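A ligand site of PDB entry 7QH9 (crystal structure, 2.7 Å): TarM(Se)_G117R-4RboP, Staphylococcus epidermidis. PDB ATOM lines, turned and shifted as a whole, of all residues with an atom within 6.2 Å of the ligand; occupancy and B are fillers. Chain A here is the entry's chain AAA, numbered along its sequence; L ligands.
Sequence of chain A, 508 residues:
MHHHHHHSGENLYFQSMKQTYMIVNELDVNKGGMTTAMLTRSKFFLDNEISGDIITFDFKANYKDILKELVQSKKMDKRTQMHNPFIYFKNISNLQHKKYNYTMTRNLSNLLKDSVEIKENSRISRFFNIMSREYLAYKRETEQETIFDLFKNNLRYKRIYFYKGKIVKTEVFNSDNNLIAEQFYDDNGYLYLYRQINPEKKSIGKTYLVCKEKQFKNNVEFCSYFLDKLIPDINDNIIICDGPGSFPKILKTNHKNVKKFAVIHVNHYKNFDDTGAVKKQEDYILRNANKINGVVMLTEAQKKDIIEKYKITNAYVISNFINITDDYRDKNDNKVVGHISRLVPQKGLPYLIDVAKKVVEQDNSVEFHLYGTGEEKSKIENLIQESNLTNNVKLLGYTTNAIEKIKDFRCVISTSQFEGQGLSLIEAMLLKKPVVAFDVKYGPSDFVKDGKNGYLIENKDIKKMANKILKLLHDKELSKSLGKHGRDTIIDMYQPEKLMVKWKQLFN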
ATOM      1  N   ILE A  23       4.600  27.024  30.427  1.00  0.00           N
ATOM      2  CA  ILE A  23       3.825  26.455  29.280  1.00  0.00           C
ATOM      3  C   ILE A  23       4.689  26.430  28.009  1.00  0.00           C
ATOM      4  O   ILE A  23       5.318  27.446  27.689  1.00  0.00           O
ATOM      5  CB  ILE A  23       2.509  27.226  29.066  1.00  0.00           C
ATOM      6  N   VAL A  24       4.681  25.307  27.292  1.00  0.00           N
ATOM      7  CA  VAL A  24       5.382  25.141  25.979  1.00  0.00           C
ATOM      8  C   VAL A  24       4.694  23.977  25.246  1.00  0.00           C
ATOM      9  O   VAL A  24       4.068  23.155  25.921  1.00  0.00           O
ATOM     10  CB  VAL A  24       6.890  24.904  26.190  1.00  0.00           C
ATOM     11  CG1 VAL A  24       7.207  23.475  26.606  1.00  0.00           C
ATOM     12  CG2 VAL A  24       7.702  25.304  24.960  1.00  0.00           C
ATOM     13  N   ASN A  25       4.788  23.926  23.911  1.00  0.00           N
ATOM     14  CA  ASN A  25       4.085  22.881  23.127  1.00  0.00           C
ATOM     15  C   ASN A  25       4.690  21.512  23.451  1.00  0.00           C
ATOM     16  O   ASN A  25       3.950  20.633  23.908  1.00  0.00           O
ATOM     17  CB  ASN A  25       4.079  23.145  21.628  1.00  0.00           C
ATOM     18  CG  ASN A  25       3.132  22.237  20.878  1.00  0.00           C
ATOM     19  OD1 ASN A  25       3.525  21.169  20.389  1.00  0.00           O
ATOM     20  ND2 ASN A  25       1.872  22.632  20.790  1.00  0.00           N
ATOM     21  N   GLU A  26       5.993  21.323  23.205  1.00  0.00           N
ATOM     22  CA  GLU A  26       6.631  20.003  23.459  1.00  0.00           C
ATOM     23  C   GLU A  26       7.912  20.129  24.289  1.00  0.00           C
ATOM     24  O   GLU A  26       8.456  21.224  24.498  1.00  0.00           O
ATOM     25  CB  GLU A  26       6.830  19.204  22.172  1.00  0.00           C
ATOM     26  CG  GLU A  26       7.798  19.810  21.152  1.00  0.00           C
ATOM     27  CD  GLU A  26       7.142  20.747  20.164  1.00  0.00           C
ATOM     28  OE1 GLU A  26       7.065  21.952  20.467  1.00  0.00           O
ATOM     29  OE2 GLU A  26       6.702  20.284  19.095  1.00  0.00           O
ATOM     30  N   LEU A  27       8.316  18.971  24.793  1.00  0.00           N
ATOM     31  CA  LEU A  27       9.513  18.767  25.627  1.00  0.00           C
ATOM     32  C   LEU A  27      10.126  17.439  25.172  1.00  0.00           C
ATOM     33  O   LEU A  27       9.375  16.441  25.053  1.00  0.00           O
ATOM     34  CB  LEU A  27       9.083  18.744  27.098  1.00  0.00           C
ATOM     35  CG  LEU A  27      10.209  18.870  28.133  1.00  0.00           C
ATOM     36  N   ASN A  30      17.734  16.777  23.101  1.00  0.00           N
ATOM     37  CA  ASN A  30      18.403  17.469  21.965  1.00  0.00           C
ATOM     38  C   ASN A  30      17.770  18.860  21.762  1.00  0.00           C
ATOM     39  O   ASN A  30      18.171  19.552  20.813  1.00  0.00           O
ATOM     40  CB  ASN A  30      18.356  16.622  20.686  1.00  0.00           C
ATOM     41  CG  ASN A  30      19.530  16.873  19.762  1.00  0.00           C
ATOM     42  OD1 ASN A  30      20.647  17.074  20.216  1.00  0.00           O
ATOM     43  ND2 ASN A  30      19.275  16.841  18.459  1.00  0.00           N
ATOM     44  N   LYS A  31      16.826  19.261  22.606  1.00  0.00           N
ATOM     45  CA  LYS A  31      16.279  20.645  22.599  1.00  0.00           C
ATOM     46  C   LYS A  31      17.051  21.441  23.662  1.00  0.00           C
ATOM     47  O   LYS A  31      16.918  21.101  24.847  1.00  0.00           O
ATOM     48  CB  LYS A  31      14.774  20.632  22.868  1.00  0.00           C
ATOM     49  N   GLY A  32      17.823  22.451  23.254  1.00  0.00           N
ATOM     50  CA  GLY A  32      18.757  23.175  24.144  1.00  0.00           C
ATOM     51  C   GLY A  32      18.458  24.656  24.249  1.00  0.00           C
ATOM     52  O   GLY A  32      19.292  25.371  24.842  1.00  0.00           O
ATOM     53  N   GLY A  33      17.325  25.132  23.730  1.00  0.00           N
ATOM     54  CA  GLY A  33      16.958  26.552  23.776  1.00  0.00           C
ATOM     55  C   GLY A  33      15.946  26.826  24.887  1.00  0.00           C
ATOM     56  O   GLY A  33      16.327  26.780  26.081  1.00  0.00           O
ATOM     57  N   MET A  34      14.708  27.113  24.496  1.00  0.00           N
ATOM     58  CA  MET A  34      13.597  27.450  25.427  1.00  0.00           C
ATOM     59  C   MET A  34      13.553  26.412  26.550  1.00  0.00           C
ATOM     60  O   MET A  34      13.519  26.804  27.719  1.00  0.00           O
ATOM     61  CB  MET A  34      12.253  27.466  24.718  1.00  0.00           C
ATOM     62  CG  MET A  34      12.094  28.600  23.729  1.00  0.00           C
ATOM     63  SD  MET A  34      10.481  28.539  22.931  1.00  0.00           S
ATOM     64  N   THR A  35      13.566  25.126  26.183  1.00  0.00           N
ATOM     65  CA  THR A  35      13.439  24.007  27.156  1.00  0.00           C
ATOM     66  C   THR A  35      14.494  24.175  28.250  1.00  0.00           C
ATOM     67  O   THR A  35      14.105  24.250  29.423  1.00  0.00           O
ATOM     68  CB  THR A  35      13.536  22.648  26.454  1.00  0.00           C
ATOM     69  OG1 THR A  35      14.755  22.642  25.708  1.00  0.00           O
ATOM     70  CG2 THR A  35      12.353  22.350  25.559  1.00  0.00           C
ATOM     71  N   THR A  36      15.769  24.283  27.880  1.00  0.00           N
ATOM     72  CA  THR A  36      16.895  24.427  28.855  1.00  0.00           C
ATOM     73  C   THR A  36      16.597  25.608  29.790  1.00  0.00           C
ATOM     74  O   THR A  36      16.671  25.410  31.012  1.00  0.00           O
ATOM     75  CB  THR A  36      18.237  24.568  28.139  1.00  0.00           C
ATOM     76  OG1 THR A  36      18.540  23.308  27.546  1.00  0.00           O
ATOM     77  CG2 THR A  36      19.365  24.985  29.060  1.00  0.00           C
ATOM     78  N   MET A  38      13.700  27.181  30.531  1.00  0.00           N
ATOM     79  CA  MET A  38      12.480  26.891  31.334  1.00  0.00           C
ATOM     80  C   MET A  38      12.813  25.924  32.468  1.00  0.00           C
ATOM     81  O   MET A  38      12.349  26.156  33.596  1.00  0.00           O
ATOM     82  CB  MET A  38      11.397  26.254  30.470  1.00  0.00           C
ATOM     83  CG  MET A  38      10.662  27.239  29.618  1.00  0.00           C
ATOM     84  SD  MET A  38       9.525  26.373  28.514  1.00  0.00           S
ATOM     85  CE  MET A  38       8.097  26.245  29.587  1.00  0.00           C
ATOM     86  N   SER A 203      -3.436  20.568   9.704  1.00  0.00           N
ATOM     87  CA  SER A 203      -3.851  21.318  10.920  1.00  0.00           C
ATOM     88  C   SER A 203      -4.860  20.530  11.767  1.00  0.00           C
ATOM     89  O   SER A 203      -5.751  19.860  11.193  1.00  0.00           O
ATOM     90  CB  SER A 203      -4.390  22.665  10.542  1.00  0.00           C
ATOM     91  N   ILE A 204      -4.743  20.640  13.096  1.00  0.00           N
ATOM     92  CA  ILE A 204      -5.672  19.999  14.083  1.00  0.00           C
ATOM     93  C   ILE A 204      -6.995  20.770  14.080  1.00  0.00           C
ATOM     94  O   ILE A 204      -6.981  21.996  14.310  1.00  0.00           O
ATOM     95  CB  ILE A 204      -5.054  19.949  15.504  1.00  0.00           C
ATOM     96  CG1 ILE A 204      -3.709  19.222  15.519  1.00  0.00           C
ATOM     97  CG2 ILE A 204      -6.030  19.329  16.493  1.00  0.00           C
ATOM     98  N   ASN A 218     -11.141  23.365  17.826  1.00  0.00           N
ATOM     99  CA  ASN A 218      -9.683  23.305  17.480  1.00  0.00           C
ATOM    100  C   ASN A 218      -8.869  22.760  18.671  1.00  0.00           C
ATOM    101  O   ASN A 218      -9.464  22.472  19.726  1.00  0.00           O
ATOM    102  CB  ASN A 218      -9.177  24.695  17.066  1.00  0.00           C
ATOM    103  CG  ASN A 218      -9.674  25.794  17.981  1.00  0.00           C
ATOM    104  OD1 ASN A 218      -9.430  25.766  19.190  1.00  0.00           O
ATOM    105  ND2 ASN A 218     -10.383  26.762  17.424  1.00  0.00           N
ATOM    106  N   ASN A 219      -7.533  22.627  18.547  1.00  0.00           N
ATOM    107  CA  ASN A 219      -6.653  22.164  19.657  1.00  0.00           C
ATOM    108  C   ASN A 219      -6.594  23.268  20.722  1.00  0.00           C
ATOM    109  O   ASN A 219      -6.591  22.923  21.919  1.00  0.00           O
ATOM    110  CB  ASN A 219      -5.250  21.778  19.180  1.00  0.00           C
ATOM    111  CG  ASN A 219      -4.362  21.165  20.258  1.00  0.00           C
ATOM    112  OD1 ASN A 219      -4.754  20.221  20.947  1.00  0.00           O
ATOM    113  ND2 ASN A 219      -3.145  21.660  20.374  1.00  0.00           N
ATOM    114  N   VAL A 220      -6.566  24.533  20.297  1.00  0.00           N
ATOM    115  CA  VAL A 220      -6.510  25.736  21.173  1.00  0.00           C
ATOM    116  C   VAL A 220      -7.658  25.674  22.200  1.00  0.00           C
ATOM    117  O   VAL A 220      -7.377  25.850  23.398  1.00  0.00           O
ATOM    118  CB  VAL A 220      -6.532  27.036  20.340  1.00  0.00           C
ATOM    119  CG1 VAL A 220      -6.439  28.278  21.222  1.00  0.00           C
ATOM    120  CG2 VAL A 220      -5.427  27.061  19.296  1.00  0.00           C
ATOM    121  N   CYS A 223      -7.143  22.641  24.745  1.00  0.00           N
ATOM    122  CA  CYS A 223      -6.019  22.943  25.654  1.00  0.00           C
ATOM    123  C   CYS A 223      -6.444  23.998  26.701  1.00  0.00           C
ATOM    124  O   CYS A 223      -6.047  23.838  27.858  1.00  0.00           O
ATOM    125  CB  CYS A 223      -4.771  23.369  24.878  1.00  0.00           C
ATOM    126  SG  CYS A 223      -4.028  22.027  23.924  1.00  0.00           S
ATOM    127  N   ASP A 242       5.868  30.449  27.875  1.00  0.00           N
ATOM    128  CA  ASP A 242       7.206  30.620  27.270  1.00  0.00           C
ATOM    129  C   ASP A 242       7.140  30.359  25.767  1.00  0.00           C
ATOM    130  O   ASP A 242       7.763  31.132  25.005  1.00  0.00           O
ATOM    131  CB  ASP A 242       8.231  29.726  27.965  1.00  0.00           C
ATOM    132  CG  ASP A 242       8.433  30.060  29.431  1.00  0.00           C
ATOM    133  OD1 ASP A 242       7.481  29.858  30.215  1.00  0.00           O
ATOM    134  OD2 ASP A 242       9.541  30.491  29.788  1.00  0.00           O
ATOM    135  N   GLY A 243       6.432  29.307  25.361  1.00  0.00           N
ATOM    136  CA  GLY A 243       6.256  28.954  23.942  1.00  0.00           C
ATOM    137  C   GLY A 243       5.421  30.007  23.216  1.00  0.00           C
ATOM    138  O   GLY A 243       4.294  30.284  23.624  1.00  0.00           O
ATOM    139  N   PRO A 244       5.951  30.648  22.146  1.00  0.00           N
ATOM    140  CA  PRO A 244       5.198  31.694  21.435  1.00  0.00           C
ATOM    141  C   PRO A 244       3.883  31.196  20.823  1.00  0.00           C
ATOM    142  O   PRO A 244       2.863  31.848  21.017  1.00  0.00           O
ATOM    143  CB  PRO A 244       6.191  32.175  20.355  1.00  0.00           C
ATOM    144  CG  PRO A 244       7.170  31.025  20.185  1.00  0.00           C
ATOM    145  CD  PRO A 244       7.290  30.416  21.570  1.00  0.00           C
ATOM    146  N   GLY A 245       3.909  30.052  20.133  1.00  0.00           N
ATOM    147  CA  GLY A 245       2.733  29.419  19.507  1.00  0.00           C
ATOM    148  C   GLY A 245       1.778  28.817  20.522  1.00  0.00           C
ATOM    149  O   GLY A 245       0.660  28.429  20.121  1.00  0.00           O
ATOM    150  N   SER A 246       2.191  28.725  21.788  1.00  0.00           N
ATOM    151  CA  SER A 246       1.360  28.169  22.885  1.00  0.00           C
ATOM    152  C   SER A 246       0.418  29.239  23.454  1.00  0.00           C
ATOM    153  O   SER A 246      -0.567  28.847  24.099  1.00  0.00           O
ATOM    154  CB  SER A 246       2.217  27.549  23.962  1.00  0.00           C
ATOM    155  OG  SER A 246       2.740  26.305  23.519  1.00  0.00           O
ATOM    156  N   PHE A 247       0.686  30.524  23.211  1.00  0.00           N
ATOM    157  CA  PHE A 247      -0.063  31.669  23.818  1.00  0.00           C
ATOM    158  C   PHE A 247      -1.575  31.644  23.552  1.00  0.00           C
ATOM    159  O   PHE A 247      -2.314  31.867  24.502  1.00  0.00           O
ATOM    160  CB  PHE A 247       0.561  33.021  23.443  1.00  0.00           C
ATOM    161  CG  PHE A 247      -0.085  34.215  24.105  1.00  0.00           C
ATOM    162  CD1 PHE A 247       0.091  34.469  25.465  1.00  0.00           C
ATOM    163  CD2 PHE A 247      -0.892  35.081  23.386  1.00  0.00           C
ATOM    164  CE1 PHE A 247      -0.511  35.562  26.070  1.00  0.00           C
ATOM    165  CE2 PHE A 247      -1.495  36.174  23.992  1.00  0.00           C
ATOM    166  CZ  PHE A 247      -1.310  36.412  25.337  1.00  0.00           C
ATOM    167  N   LYS A 249      -3.770  29.386  23.422  1.00  0.00           N
ATOM    168  CA  LYS A 249      -4.317  28.389  24.385  1.00  0.00           C
ATOM    169  C   LYS A 249      -4.360  28.971  25.802  1.00  0.00           C
ATOM    170  O   LYS A 249      -5.139  28.457  26.618  1.00  0.00           O
ATOM    171  CB  LYS A 249      -3.451  27.113  24.375  1.00  0.00           C
ATOM    172  CG  LYS A 249      -3.416  26.386  23.046  1.00  0.00           C
ATOM    173  CD  LYS A 249      -2.265  25.426  22.906  1.00  0.00           C
ATOM    174  CE  LYS A 249      -2.202  24.780  21.539  1.00  0.00           C
ATOM    175  NZ  LYS A 249      -1.769  25.745  20.491  1.00  0.00           N
ATOM    176  N   GLN A 281       3.839  35.309  15.186  1.00  0.00           N
ATOM    177  CA  GLN A 281       3.624  34.607  16.487  1.00  0.00           C
ATOM    178  C   GLN A 281       3.824  35.613  17.632  1.00  0.00           C
ATOM    179  O   GLN A 281       2.912  35.734  18.472  1.00  0.00           O
ATOM    180  CB  GLN A 281       4.577  33.428  16.612  1.00  0.00           C
ATOM    181  CG  GLN A 281       3.952  32.195  17.234  1.00  0.00           C
ATOM    182  CD  GLN A 281       4.762  30.960  16.939  1.00  0.00           C
ATOM    183  OE1 GLN A 281       5.988  30.963  17.030  1.00  0.00           O
ATOM    184  NE2 GLN A 281       4.080  29.898  16.549  1.00  0.00           N
HETATM  185  O1  LIG L   1      -2.829  25.870  16.584  1.00  0.00           O
HETATM  186  P1  LIG L   1      -2.452  24.375  17.086  1.00  0.00           P
HETATM  187  O2  LIG L   1      -3.200  23.366  16.075  1.00  0.00           O
HETATM  188  O3  LIG L   1      -2.871  24.159  18.499  1.00  0.00           O
HETATM  189  O4  LIG L   1      -0.865  24.133  16.873  1.00  0.00           O
HETATM  190  C1  LIG L   1      -0.075  24.930  15.976  1.00  0.00           C
HETATM  191  C2  LIG L   1       0.933  25.759  16.785  1.00  0.00           C
HETATM  192  O5  LIG L   1       1.187  26.990  16.066  1.00  0.00           O
HETATM  193  C3  LIG L   1       2.239  24.962  17.007  1.00  0.00           C
HETATM  194  O6  LIG L   1       1.992  23.932  17.984  1.00  0.00           O
HETATM  195  C4  LIG L   1       3.406  25.877  17.466  1.00  0.00           C
HETATM  196  O7  LIG L   1       4.260  26.139  16.333  1.00  0.00           O
HETATM  197  C5  LIG L   1       4.251  25.257  18.572  1.00  0.00           C
HETATM  198  O8  LIG L   1       4.108  26.120  19.723  1.00  0.00           O
HETATM  199  P2  LIG L   1       5.405  26.556  20.564  1.00  0.00           P
HETATM  200  O9  LIG L   1       4.880  26.706  22.066  1.00  0.00           O
HETATM  201  O10 LIG L   1       6.003  27.794  20.012  1.00  0.00           O
HETATM  202  O11 LIG L   1       6.404  25.311  20.589  1.00  0.00           O
HETATM  203  C6  LIG L   1       7.723  25.436  21.129  1.00  0.00           C
HETATM  204  C7  LIG L   1       8.763  25.199  20.020  1.00  0.00           C
HETATM  205  O12 LIG L   1       8.428  23.971  19.340  1.00  0.00           O
HETATM  206  C8  LIG L   1      10.225  25.208  20.555  1.00  0.00           C
HETATM  207  O13 LIG L   1      11.123  25.183  19.420  1.00  0.00           O
HETATM  208  C9  LIG L   1      10.509  24.069  21.585  1.00  0.00           C
HETATM  209  O14 LIG L   1      10.169  24.501  22.922  1.00  0.00           O
HETATM  210  C10 LIG L   1      11.953  23.540  21.654  1.00  0.00           C
HETATM  211  O15 LIG L   1      12.900  24.583  21.341  1.00  0.00           O
HETATM  212  P3  LIG L   1      14.462  24.454  21.770  1.00  0.00           P
HETATM  213  O16 LIG L   1      15.003  23.111  21.060  1.00  0.00           O
HETATM  214  O17 LIG L   1      14.631  24.458  23.246  1.00  0.00           O
HETATM  215  O18 LIG L   1      15.214  25.682  21.044  1.00  0.00           O
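An oxygen (O9) of the ligand sits at hydrogen-bond distance from the backbone NH (N) of Ser 246 (3.4 Å). An oxygen (O9) of the ligand is in hydrogen-bond range of the side-chain hydroxyl of Ser 246, at 2.6 Å. OE1 of Glu 26 lies within hydrogen-bond range of O12 of the ligand (2.7 Å). NZ of Lys 249 is in salt-bridge range of O3 of the ligand (2.8 Å). The backbone NH of Gly 33 sits at hydrogen-bond distance from an oxygen (O17) of the ligand, at 2.8 Å. O17 of the ligand is in hydrogen-bond range of N of Met 34 (2.9 Å). N of Thr 35 sits at hydrogen-bond distance from O17 of the ligand, at 3.2 Å. The side-chain hydroxyl of Thr 35 is in hydrogen-bond range of an oxygen (O17) of the ligand, at 3.1 Å. An oxygen (O10) of the ligand sits at hydrogen-bond distance from the backbone NH of Gly 245, 3.1 Å away. The backbone NH of Asn 25 sits at hydrogen-bond distance from an oxygen (O9) of the ligand (3.3 Å). The side-chain amide nitrogen (ND2) of Asn 25 is in hydrogen-bond range of an oxygen (O6) of the ligand (3.1 Å). O3 of the ligand sits at hydrogen-bond distance from ND2 of Asn 219.
The side-chain hydroxyl of Ser 246 lies within hydrogen-bond range of the backbone NH of Asn 25 (3.2 Å). The side-chain hydroxyl (OG1) of Thr 35 lies within hydrogen-bond range of the backbone carbonyl oxygen (O) of Lys 31, at 2.8 Å. The backbone carbonyl oxygen (O) of Asn 219 lies within hydrogen-bond range of the side-chain sulfur (SG) of Cys 223. The backbone NH (N) of Gly 243 is in hydrogen-bond range of the backbone carbonyl oxygen (O) of Ile 23, 3.2 Å away. The side-chain hydroxyl (OG1) of Thr 36 lies close to the backbone carbonyl oxygen (O) of Gly 32 (3.5 Å). The side-chain amide oxygen of Asn 218 lies within hydrogen-bond range of the backbone NH of Val 220 (3.3 Å).
Val 24 touches the ligand (CG2 to O14, 3.3 Å). CB of Lys 31 touches O16 of the ligand (3.1 Å). N of Gly 32 touches O16 of the ligand, 3.6 Å away. Ile 204 touches the ligand. Val 220 touches the ligand (CG2 to O1, 3.9 Å). Gly 243 touches the ligand (CA to O9, 3.2 Å). Pro 244 touches the ligand (CD to O10, 3.3 Å). NE2 of Gln 281 touches O7 of the ligand (3.8 Å). Of the 27 residues printed, 17 come within 4 Å of the ligand.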
